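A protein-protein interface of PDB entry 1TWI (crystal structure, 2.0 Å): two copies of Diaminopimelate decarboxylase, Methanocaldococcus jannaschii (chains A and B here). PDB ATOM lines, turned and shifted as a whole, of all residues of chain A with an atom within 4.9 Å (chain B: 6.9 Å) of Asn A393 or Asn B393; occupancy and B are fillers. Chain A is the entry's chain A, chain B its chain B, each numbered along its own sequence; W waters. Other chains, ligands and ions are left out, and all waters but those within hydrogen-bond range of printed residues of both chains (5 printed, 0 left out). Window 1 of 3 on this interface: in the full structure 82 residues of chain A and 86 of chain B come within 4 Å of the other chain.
The backbone carbonyl oxygen of Arg B398 lies close to the side-chain amide oxygen of Asn B394. The side-chain amide oxygen (OD1) of Asn A394 lies close to the backbone carbonyl oxygen (O) of Arg A398 (2.9 Å). The backbone carbonyl oxygen of Asn A325 lies within hydrogen-bond range of the backbone NH of Asn A393, 2.8 Å away. O of Asn B325 is in hydrogen-bond range of N of Asn B393, at 2.9 Å. The side-chain amide oxygen (OD1) of Asn B394 lies close to the side-chain carboxylate (OE1) of Glu B418 (2.9 Å). The side-chain sulfur (SD) of Met A328 lies close to the side-chain amide oxygen (OD1) of Asn A393, at 3.4 Å.
Of the 10 printed residues of chain A, 6 touch a printed residue of chain B. Printed residues of chain A that touch a printed residue of chain B: Met A391, Ala A392, Asn A393, Asn A394, Tyr A395 and Arg A400. Of the 20 printed residues of chain B, 7 touch a printed residue of chain A. Hydrophobic or aromatic side chains of chain B that line the printed part of chain A: Met B391 and Tyr B395. Among the printed residues, 9 pairs touch across the chains. Among the printed residues, no Asp or Glu carboxylate lies within 4 Å of a Lys or Arg side-chain nitrogen of the other chain.
Water W3 lies within hydrogen-bond range of O of Ala A392 (2.6 Å) and N of Asn B394 (2.7 Å). Water W4 lies within hydrogen-bond range of the backbone carbonyl oxygen (O) of Ala B392 (2.7 Å), the backbone NH (N) of Asn A394 (2.7 Å) and the backbone carbonyl oxygen (O) of Ser B390 (3.2 Å). Water W2 bridges the guanidinium group of Arg B400 (2.8 Å) and the side-chain amide nitrogen of Asn A394 (2.8 Å). Water W1 bridges O of Ser B390 and O of Asn A394. Water W5 lies within hydrogen-bond range of ND2 of Asn B394 (2.9 Å), NH2 of Arg A400 (2.9 Å) and OE2 of Glu B418 (2.9 Å).
NH2 of Arg A400 lies close to NH2 of Arg B400 (3.4 Å). ND2 of Asn B394 sits close to NH1 of Arg A400. The guanidinium group (NH1) of Arg B400 lies close to the side-chain amide nitrogen (ND2) of Asn A394, 2.7 Å away.
Met A391 touches Tyr B395, and with the chains exchanged Tyr A395 touches Met B391. Ala A392 touches Asn B393, and with the chains exchanged Asn A393 touches Ala B392. Asn A394 touches Arg B400, and with the chains exchanged Arg A400 touches Asn B394. Arg B400 touches its own counterpart, Arg A400. Positions printed for both chains: 324, 325, 328, 391, 392, 393, 394, 395, 398 and 400.
Among the printed residues, merely in contact across the chains: Met A391 with Tyr B395, Ala A392 with Asn B393, Asn A393 with Ala B392, Asn A393 with Asn B393, Tyr A395 with Ser B390 and Tyr A395 with Met B391.
Asn A393 touches two residues of chain B. Asn B393 touches two residues of chain A. Of the printed residues of chain A, Tyr B395 touches Met A391 (3.5 Å). Of the printed residues of chain A, Ser B390 touches Tyr A395. Printed residues of chain B within 4 Å of Met A391: Tyr B395. Of the printed residues of chain B, Ala A392 touches Asn B393 (3.5 Å). Printed residues of chain B within 4 Å of Tyr A395: Ser B390 and Met B391. The nearest residue of chain B that does not touch Asn A393 is Met B391 (4.3 Å). The nearest printed residue of chain A that does not touch Asn B394 is Ala A392 (4.6 Å).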
ATOM      1  N   MET A 324      19.707   6.629  17.693  1.00  0.00           N
ATOM      2  CA  MET A 324      19.114   7.208  18.888  1.00  0.00           C
ATOM      3  C   MET A 324      20.151   7.740  19.915  1.00  0.00           C
ATOM      4  O   MET A 324      19.839   8.675  20.659  1.00  0.00           O
ATOM      5  CB  MET A 324      18.181   6.188  19.562  1.00  0.00           C
ATOM      6  CG  MET A 324      18.900   4.946  20.113  1.00  0.00           C
ATOM      7  SD  MET A 324      17.732   3.795  20.875  1.00  0.00           S
ATOM      8  CE  MET A 324      17.555   4.504  22.566  1.00  0.00           C
ATOM      9  N   ASN A 325      21.343   7.148  19.988  1.00  0.00           N
ATOM     10  CA  ASN A 325      22.343   7.662  20.949  1.00  0.00           C
ATOM     11  C   ASN A 325      22.795   9.121  20.525  1.00  0.00           C
ATOM     12  O   ASN A 325      23.242   9.946  21.354  1.00  0.00           O
ATOM     13  CB  ASN A 325      23.564   6.717  20.983  1.00  0.00           C
ATOM     14  CG  ASN A 325      24.356   6.764  19.681  1.00  0.00           C
ATOM     15  OD1 ASN A 325      23.887   6.297  18.613  1.00  0.00           O
ATOM     16  ND2 ASN A 325      25.551   7.358  19.749  1.00  0.00           N
ATOM     17  N   MET A 328      18.021  11.412  20.694  1.00  0.00           N
ATOM     18  CA  MET A 328      17.062  10.549  21.365  1.00  0.00           C
ATOM     19  C   MET A 328      15.581  10.871  21.240  1.00  0.00           C
ATOM     20  O   MET A 328      14.762  10.067  21.720  1.00  0.00           O
ATOM     21  CB  MET A 328      17.384  10.531  22.864  1.00  0.00           C
ATOM     22  CG  MET A 328      18.755   9.918  23.201  1.00  0.00           C
ATOM     23  SD  MET A 328      18.579   8.095  23.177  1.00  0.00           S
ATOM     24  CE  MET A 328      17.841   7.939  24.846  1.00  0.00           C
ATOM     25  N   MET A 391      21.047  15.506  24.956  1.00  0.00           N
ATOM     26  CA  MET A 391      20.636  14.221  25.550  1.00  0.00           C
ATOM     27  C   MET A 391      21.392  13.081  24.879  1.00  0.00           C
ATOM     28  O   MET A 391      21.082  11.916  25.130  1.00  0.00           O
ATOM     29  CB  MET A 391      19.109  13.997  25.392  1.00  0.00           C
ATOM     30  CG  MET A 391      18.255  15.114  26.055  1.00  0.00           C
ATOM     31  SD  MET A 391      16.444  14.850  26.133  1.00  0.00           S
ATOM     32  CE  MET A 391      16.326  13.628  27.355  1.00  0.00           C
ATOM     33  N   ALA A 392      22.374  13.382  24.030  1.00  0.00           N
ATOM     34  CA  ALA A 392      23.102  12.301  23.327  1.00  0.00           C
ATOM     35  C   ALA A 392      23.835  11.401  24.333  1.00  0.00           C
ATOM     36  O   ALA A 392      24.175  11.856  25.437  1.00  0.00           O
ATOM     37  CB  ALA A 392      24.124  12.919  22.338  1.00  0.00           C
ATOM     38  N   ASN A 393      24.109  10.144  23.982  1.00  0.00           N
ATOM     39  CA  ASN A 393      24.804   9.309  24.941  1.00  0.00           C
ATOM     40  C   ASN A 393      25.651   8.297  24.176  1.00  0.00           C
ATOM     41  O   ASN A 393      25.745   8.405  22.977  1.00  0.00           O
ATOM     42  CB  ASN A 393      23.771   8.606  25.785  1.00  0.00           C
ATOM     43  CG  ASN A 393      22.722   7.934  24.929  1.00  0.00           C
ATOM     44  OD1 ASN A 393      21.546   8.366  24.879  1.00  0.00           O
ATOM     45  ND2 ASN A 393      23.115   6.905  24.240  1.00  0.00           N
ATOM     46  N   ASN A 394      26.240   7.321  24.861  1.00  0.00           N
ATOM     47  CA  ASN A 394      27.105   6.340  24.222  1.00  0.00           C
ATOM     48  C   ASN A 394      26.458   4.968  24.128  1.00  0.00           C
ATOM     49  O   ASN A 394      27.156   3.939  23.984  1.00  0.00           O
ATOM     50  CB  ASN A 394      28.419   6.199  25.013  1.00  0.00           C
ATOM     51  CG  ASN A 394      29.302   7.439  24.908  1.00  0.00           C
ATOM     52  OD1 ASN A 394      29.506   7.999  23.808  1.00  0.00           O
ATOM     53  ND2 ASN A 394      29.858   7.848  26.016  1.00  0.00           N
ATOM     54  N   TYR A 395      25.136   4.926  24.195  1.00  0.00           N
ATOM     55  CA  TYR A 395      24.454   3.632  24.119  1.00  0.00           C
ATOM     56  C   TYR A 395      24.894   2.800  22.917  1.00  0.00           C
ATOM     57  O   TYR A 395      25.032   3.335  21.805  1.00  0.00           O
ATOM     58  CB  TYR A 395      22.935   3.849  24.126  1.00  0.00           C
ATOM     59  CG  TYR A 395      22.134   2.581  24.219  1.00  0.00           C
ATOM     60  CD1 TYR A 395      22.451   1.596  25.157  1.00  0.00           C
ATOM     61  CD2 TYR A 395      20.990   2.410  23.415  1.00  0.00           C
ATOM     62  CE1 TYR A 395      21.631   0.446  25.309  1.00  0.00           C
ATOM     63  CE2 TYR A 395      20.177   1.296  23.537  1.00  0.00           C
ATOM     64  CZ  TYR A 395      20.511   0.306  24.501  1.00  0.00           C
ATOM     65  OH  TYR A 395      19.726  -0.823  24.607  1.00  0.00           O
ATOM     66  N   ARG A 398      28.767   3.716  21.179  1.00  0.00           N
ATOM     67  CA  ARG A 398      28.917   4.541  19.980  1.00  0.00           C
ATOM     68  C   ARG A 398      29.339   5.927  20.467  1.00  0.00           C
ATOM     69  O   ARG A 398      28.736   6.464  21.413  1.00  0.00           O
ATOM     70  CB  ARG A 398      27.572   4.669  19.238  1.00  0.00           C
ATOM     71  CG  ARG A 398      27.122   3.436  18.537  1.00  0.00           C
ATOM     72  CD  ARG A 398      25.712   3.638  17.964  1.00  0.00           C
ATOM     73  NE  ARG A 398      25.485   2.458  17.154  1.00  0.00           N
ATOM     74  CZ  ARG A 398      25.513   2.452  15.827  1.00  0.00           C
ATOM     75  NH1 ARG A 398      25.721   3.616  15.180  1.00  0.00           N
ATOM     76  NH2 ARG A 398      25.443   1.275  15.179  1.00  0.00           N
ATOM     77  N   ARG A 400      29.768  10.003  20.762  1.00  0.00           N
ATOM     78  CA  ARG A 400      28.839  11.094  20.447  1.00  0.00           C
ATOM     79  C   ARG A 400      29.414  11.723  19.198  1.00  0.00           C
ATOM     80  O   ARG A 400      30.640  11.786  19.002  1.00  0.00           O
ATOM     81  CB  ARG A 400      28.676  12.053  21.626  1.00  0.00           C
ATOM     82  CG  ARG A 400      27.708  11.390  22.668  1.00  0.00           C
ATOM     83  CD  ARG A 400      27.696  12.121  23.978  1.00  0.00           C
ATOM     84  NE  ARG A 400      28.980  11.982  24.673  1.00  0.00           N
ATOM     85  CZ  ARG A 400      29.258  12.597  25.824  1.00  0.00           C
ATOM     86  NH1 ARG A 400      28.341  13.377  26.397  1.00  0.00           N
ATOM     87  NH2 ARG A 400      30.450  12.468  26.394  1.00  0.00           N
ATOM     88  N   MET B 324      17.948  11.013  36.269  1.00  0.00           N
ATOM     89  CA  MET B 324      17.689  10.238  35.065  1.00  0.00           C
ATOM     90  C   MET B 324      18.914  10.171  34.158  1.00  0.00           C
ATOM     91  O   MET B 324      19.053   9.187  33.410  1.00  0.00           O
ATOM     92  CB  MET B 324      16.486  10.796  34.299  1.00  0.00           C
ATOM     93  CG  MET B 324      16.755  12.199  33.707  1.00  0.00           C
ATOM     94  SD  MET B 324      15.265  12.823  32.786  1.00  0.00           S
ATOM     95  CE  MET B 324      15.504  12.090  31.025  1.00  0.00           C
ATOM     96  N   ASN B 325      19.792  11.189  34.173  1.00  0.00           N
ATOM     97  CA  ASN B 325      20.998  11.104  33.300  1.00  0.00           C
ATOM     98  C   ASN B 325      21.917   9.986  33.837  1.00  0.00           C
ATOM     99  O   ASN B 325      22.747   9.466  33.109  1.00  0.00           O
ATOM    100  CB  ASN B 325      21.789  12.403  33.303  1.00  0.00           C
ATOM    101  CG  ASN B 325      22.446  12.660  34.655  1.00  0.00           C
ATOM    102  OD1 ASN B 325      21.771  12.747  35.682  1.00  0.00           O
ATOM    103  ND2 ASN B 325      23.776  12.757  34.653  1.00  0.00           N
ATOM    104  N   ASP B 326      21.820   9.660  35.133  1.00  0.00           N
ATOM    105  CA  ASP B 326      22.620   8.555  35.659  1.00  0.00           C
ATOM    106  C   ASP B 326      22.018   7.190  35.328  1.00  0.00           C
ATOM    107  O   ASP B 326      22.736   6.171  35.206  1.00  0.00           O
ATOM    108  CB  ASP B 326      22.682   8.635  37.201  1.00  0.00           C
ATOM    109  CG  ASP B 326      23.264   9.932  37.666  1.00  0.00           C
ATOM    110  OD1 ASP B 326      24.386  10.252  37.160  1.00  0.00           O
ATOM    111  OD2 ASP B 326      22.621  10.636  38.497  1.00  0.00           O
ATOM    112  N   MET B 327      20.687   7.147  35.270  1.00  0.00           N
ATOM    113  CA  MET B 327      19.978   5.896  35.072  1.00  0.00           C
ATOM    114  C   MET B 327      18.626   6.277  34.505  1.00  0.00           C
ATOM    115  O   MET B 327      17.756   6.807  35.203  1.00  0.00           O
ATOM    116  CB  MET B 327      19.882   5.157  36.426  1.00  0.00           C
ATOM    117  CG  MET B 327      19.741   3.633  36.324  1.00  0.00           C
ATOM    118  SD  MET B 327      18.071   3.123  35.850  1.00  0.00           S
ATOM    119  CE  MET B 327      17.157   3.388  37.425  1.00  0.00           C
ATOM    120  N   MET B 328      18.475   5.964  33.224  1.00  0.00           N
ATOM    121  CA  MET B 328      17.330   6.397  32.408  1.00  0.00           C
ATOM    122  C   MET B 328      16.038   5.564  32.363  1.00  0.00           C
ATOM    123  O   MET B 328      15.025   6.052  31.821  1.00  0.00           O
ATOM    124  CB  MET B 328      17.826   6.546  30.952  1.00  0.00           C
ATOM    125  CG  MET B 328      18.823   7.697  30.700  1.00  0.00           C
ATOM    126  SD  MET B 328      17.954   9.339  30.662  1.00  0.00           S
ATOM    127  CE  MET B 328      17.345   9.288  28.902  1.00  0.00           C
ATOM    128  N   LEU B 357      16.941  16.778  37.917  1.00  0.00           N
ATOM    129  CA  LEU B 357      16.871  17.381  36.576  1.00  0.00           C
ATOM    130  C   LEU B 357      15.556  18.104  36.339  1.00  0.00           C
ATOM    131  O   LEU B 357      14.517  17.735  36.930  1.00  0.00           O
ATOM    132  CB  LEU B 357      17.107  16.322  35.486  1.00  0.00           C
ATOM    133  CG  LEU B 357      18.597  16.016  35.459  1.00  0.00           C
ATOM    134  CD1 LEU B 357      18.940  15.035  36.658  1.00  0.00           C
ATOM    135  CD2 LEU B 357      18.956  15.381  34.090  1.00  0.00           C
ATOM    136  N   GLY B 388      21.908   0.716  32.597  1.00  0.00           N
ATOM    137  CA  GLY B 388      22.040   1.748  33.620  1.00  0.00           C
ATOM    138  C   GLY B 388      23.175   2.679  33.149  1.00  0.00           C
ATOM    139  O   GLY B 388      22.927   3.686  32.428  1.00  0.00           O
ATOM    140  N   ILE B 389      24.430   2.353  33.479  1.00  0.00           N
ATOM    141  CA  ILE B 389      25.530   3.206  33.027  1.00  0.00           C
ATOM    142  C   ILE B 389      25.573   3.195  31.507  1.00  0.00           C
ATOM    143  O   ILE B 389      25.971   4.216  30.898  1.00  0.00           O
ATOM    144  CB  ILE B 389      26.963   2.764  33.583  1.00  0.00           C
ATOM    145  CG1 ILE B 389      28.035   3.891  33.356  1.00  0.00           C
ATOM    146  CG2 ILE B 389      27.480   1.472  32.868  1.00  0.00           C
ATOM    147  CD1 ILE B 389      27.746   5.184  34.161  1.00  0.00           C
ATOM    148  N   SER B 390      25.162   2.085  30.876  1.00  0.00           N
ATOM    149  CA  SER B 390      25.255   2.050  29.416  1.00  0.00           C
ATOM    150  C   SER B 390      24.339   3.057  28.717  1.00  0.00           C
ATOM    151  O   SER B 390      24.546   3.355  27.549  1.00  0.00           O
ATOM    152  CB  SER B 390      25.019   0.639  28.818  1.00  0.00           C
ATOM    153  OG  SER B 390      23.651   0.276  28.948  1.00  0.00           O
ATOM    154  N   MET B 391      23.354   3.603  29.421  1.00  0.00           N
ATOM    155  CA  MET B 391      22.511   4.596  28.786  1.00  0.00           C
ATOM    156  C   MET B 391      22.684   5.944  29.540  1.00  0.00           C
ATOM    157  O   MET B 391      21.953   6.910  29.277  1.00  0.00           O
ATOM    158  CB  MET B 391      21.038   4.152  28.825  1.00  0.00           C
ATOM    159  CG  MET B 391      20.771   2.883  28.033  1.00  0.00           C
ATOM    160  SD  MET B 391      18.992   2.509  27.868  1.00  0.00           S
ATOM    161  CE  MET B 391      18.635   3.757  26.618  1.00  0.00           C
ATOM    162  N   ALA B 392      23.645   6.037  30.448  1.00  0.00           N
ATOM    163  CA  ALA B 392      23.831   7.298  31.138  1.00  0.00           C
ATOM    164  C   ALA B 392      24.278   8.425  30.168  1.00  0.00           C
ATOM    165  O   ALA B 392      24.876   8.179  29.107  1.00  0.00           O
ATOM    166  CB  ALA B 392      24.877   7.140  32.299  1.00  0.00           C
ATOM    167  N   ASN B 393      24.035   9.685  30.531  1.00  0.00           N
ATOM    168  CA  ASN B 393      24.363  10.767  29.599  1.00  0.00           C
ATOM    169  C   ASN B 393      24.641  12.016  30.424  1.00  0.00           C
ATOM    170  O   ASN B 393      24.623  11.951  31.657  1.00  0.00           O
ATOM    171  CB  ASN B 393      23.167  11.035  28.669  1.00  0.00           C
ATOM    172  CG  ASN B 393      21.866  11.192  29.456  1.00  0.00           C
ATOM    173  OD1 ASN B 393      21.004  10.267  29.495  1.00  0.00           O
ATOM    174  ND2 ASN B 393      21.742  12.298  30.145  1.00  0.00           N
ATOM    175  N   ASN B 394      24.860  13.145  29.764  1.00  0.00           N
ATOM    176  CA  ASN B 394      25.147  14.386  30.496  1.00  0.00           C
ATOM    177  C   ASN B 394      23.994  15.401  30.518  1.00  0.00           C
ATOM    178  O   ASN B 394      24.243  16.579  30.725  1.00  0.00           O
ATOM    179  CB  ASN B 394      26.379  15.082  29.900  1.00  0.00           C
ATOM    180  CG  ASN B 394      27.642  14.254  30.072  1.00  0.00           C
ATOM    181  OD1 ASN B 394      28.007  13.832  31.202  1.00  0.00           O
ATOM    182  ND2 ASN B 394      28.302  13.992  28.968  1.00  0.00           N
ATOM    183  N   TYR B 395      22.766  14.954  30.260  1.00  0.00           N
ATOM    184  CA  TYR B 395      21.625  15.886  30.266  1.00  0.00           C
ATOM    185  C   TYR B 395      21.616  16.753  31.546  1.00  0.00           C
ATOM    186  O   TYR B 395      21.913  16.263  32.660  1.00  0.00           O
ATOM    187  CB  TYR B 395      20.353  15.074  30.117  1.00  0.00           C
ATOM    188  CG  TYR B 395      19.125  15.892  29.900  1.00  0.00           C
ATOM    189  CD1 TYR B 395      19.079  16.888  28.939  1.00  0.00           C
ATOM    190  CD2 TYR B 395      17.963  15.603  30.620  1.00  0.00           C
ATOM    191  CE1 TYR B 395      17.879  17.581  28.687  1.00  0.00           C
ATOM    192  CE2 TYR B 395      16.783  16.286  30.376  1.00  0.00           C
ATOM    193  CZ  TYR B 395      16.766  17.275  29.400  1.00  0.00           C
ATOM    194  OH  TYR B 395      15.607  17.953  29.193  1.00  0.00           O
ATOM    195  N   ASN B 396      21.327  18.035  31.346  1.00  0.00           N
ATOM    196  CA  ASN B 396      21.335  19.108  32.376  1.00  0.00           C
ATOM    197  C   ASN B 396      22.792  19.405  32.782  1.00  0.00           C
ATOM    198  O   ASN B 396      23.033  19.916  33.875  1.00  0.00           O
ATOM    199  CB  ASN B 396      20.520  18.732  33.624  1.00  0.00           C
ATOM    200  CG  ASN B 396      19.013  18.888  33.430  1.00  0.00           C
ATOM    201  OD1 ASN B 396      18.287  19.086  34.409  1.00  0.00           O
ATOM    202  ND2 ASN B 396      18.535  18.783  32.197  1.00  0.00           N
ATOM    203  N   ARG B 398      25.302  17.382  33.640  1.00  0.00           N
ATOM    204  CA  ARG B 398      25.679  16.645  34.841  1.00  0.00           C
ATOM    205  C   ARG B 398      26.705  15.564  34.413  1.00  0.00           C
ATOM    206  O   ARG B 398      26.471  14.863  33.432  1.00  0.00           O
ATOM    207  CB  ARG B 398      24.405  15.977  35.435  1.00  0.00           C
ATOM    208  CG  ARG B 398      23.473  17.029  36.101  1.00  0.00           C
ATOM    209  CD  ARG B 398      22.077  16.461  36.321  1.00  0.00           C
ATOM    210  NE  ARG B 398      22.109  15.805  37.602  1.00  0.00           N
ATOM    211  CZ  ARG B 398      21.755  16.427  38.732  1.00  0.00           C
ATOM    212  NH1 ARG B 398      21.292  17.700  38.755  1.00  0.00           N
ATOM    213  NH2 ARG B 398      22.016  15.837  39.851  1.00  0.00           N
ATOM    214  N   GLY B 399      27.816  15.403  35.120  1.00  0.00           N
ATOM    215  CA  GLY B 399      28.760  14.383  34.691  1.00  0.00           C
ATOM    216  C   GLY B 399      28.203  13.001  34.984  1.00  0.00           C
ATOM    217  O   GLY B 399      27.354  12.860  35.895  1.00  0.00           O
ATOM    218  N   ARG B 400      28.628  11.993  34.210  1.00  0.00           N
ATOM    219  CA  ARG B 400      28.229  10.603  34.464  1.00  0.00           C
ATOM    220  C   ARG B 400      28.928  10.204  35.805  1.00  0.00           C
ATOM    221  O   ARG B 400      30.049  10.633  36.097  1.00  0.00           O
ATOM    222  CB  ARG B 400      28.611   9.760  33.263  1.00  0.00           C
ATOM    223  CG  ARG B 400      27.571   9.984  32.108  1.00  0.00           C
ATOM    224  CD  ARG B 400      27.962   9.317  30.834  1.00  0.00           C
ATOM    225  NE  ARG B 400      29.163   9.949  30.303  1.00  0.00           N
ATOM    226  CZ  ARG B 400      29.781   9.502  29.221  1.00  0.00           C
ATOM    227  NH1 ARG B 400      29.285   8.432  28.604  1.00  0.00           N
ATOM    228  NH2 ARG B 400      30.882  10.094  28.769  1.00  0.00           N
ATOM    229  N   PRO B 401      28.259   9.391  36.633  1.00  0.00           N
ATOM    230  CA  PRO B 401      28.803   8.985  37.934  1.00  0.00           C
ATOM    231  C   PRO B 401      29.928   7.978  38.039  1.00  0.00           C
ATOM    232  O   PRO B 401      30.296   7.293  37.065  1.00  0.00           O
ATOM    233  CB  PRO B 401      27.577   8.489  38.645  1.00  0.00           C
ATOM    234  CG  PRO B 401      26.799   7.773  37.519  1.00  0.00           C
ATOM    235  CD  PRO B 401      27.062   8.597  36.266  1.00  0.00           C
ATOM    236  N   GLU B 418      32.819  12.257  35.937  1.00  0.00           N
ATOM    237  CA  GLU B 418      33.196  13.378  35.033  1.00  0.00           C
ATOM    238  C   GLU B 418      33.151  14.712  35.780  1.00  0.00           C
ATOM    239  O   GLU B 418      32.221  14.952  36.557  1.00  0.00           O
ATOM    240  CB  GLU B 418      32.234  13.433  33.851  1.00  0.00           C
ATOM    241  CG  GLU B 418      32.418  12.242  32.971  1.00  0.00           C
ATOM    242  CD  GLU B 418      31.454  12.202  31.830  1.00  0.00           C
ATOM    243  OE1 GLU B 418      30.220  12.208  32.070  1.00  0.00           O
ATOM    244  OE2 GLU B 418      31.940  12.158  30.682  1.00  0.00           O
HETATM  245  O   HOH W   1      27.313   3.312  26.797  1.00  0.00           O
HETATM  246  O   HOH W   2      32.263   9.134  26.582  1.00  0.00           O
HETATM  247  O   HOH W   3      24.687  13.785  27.106  1.00  0.00           O
HETATM  248  O   HOH W   4      25.781   6.348  27.387  1.00  0.00           O
HETATM  249  O   HOH W   5      31.187  14.148  28.662  1.00  0.00           O
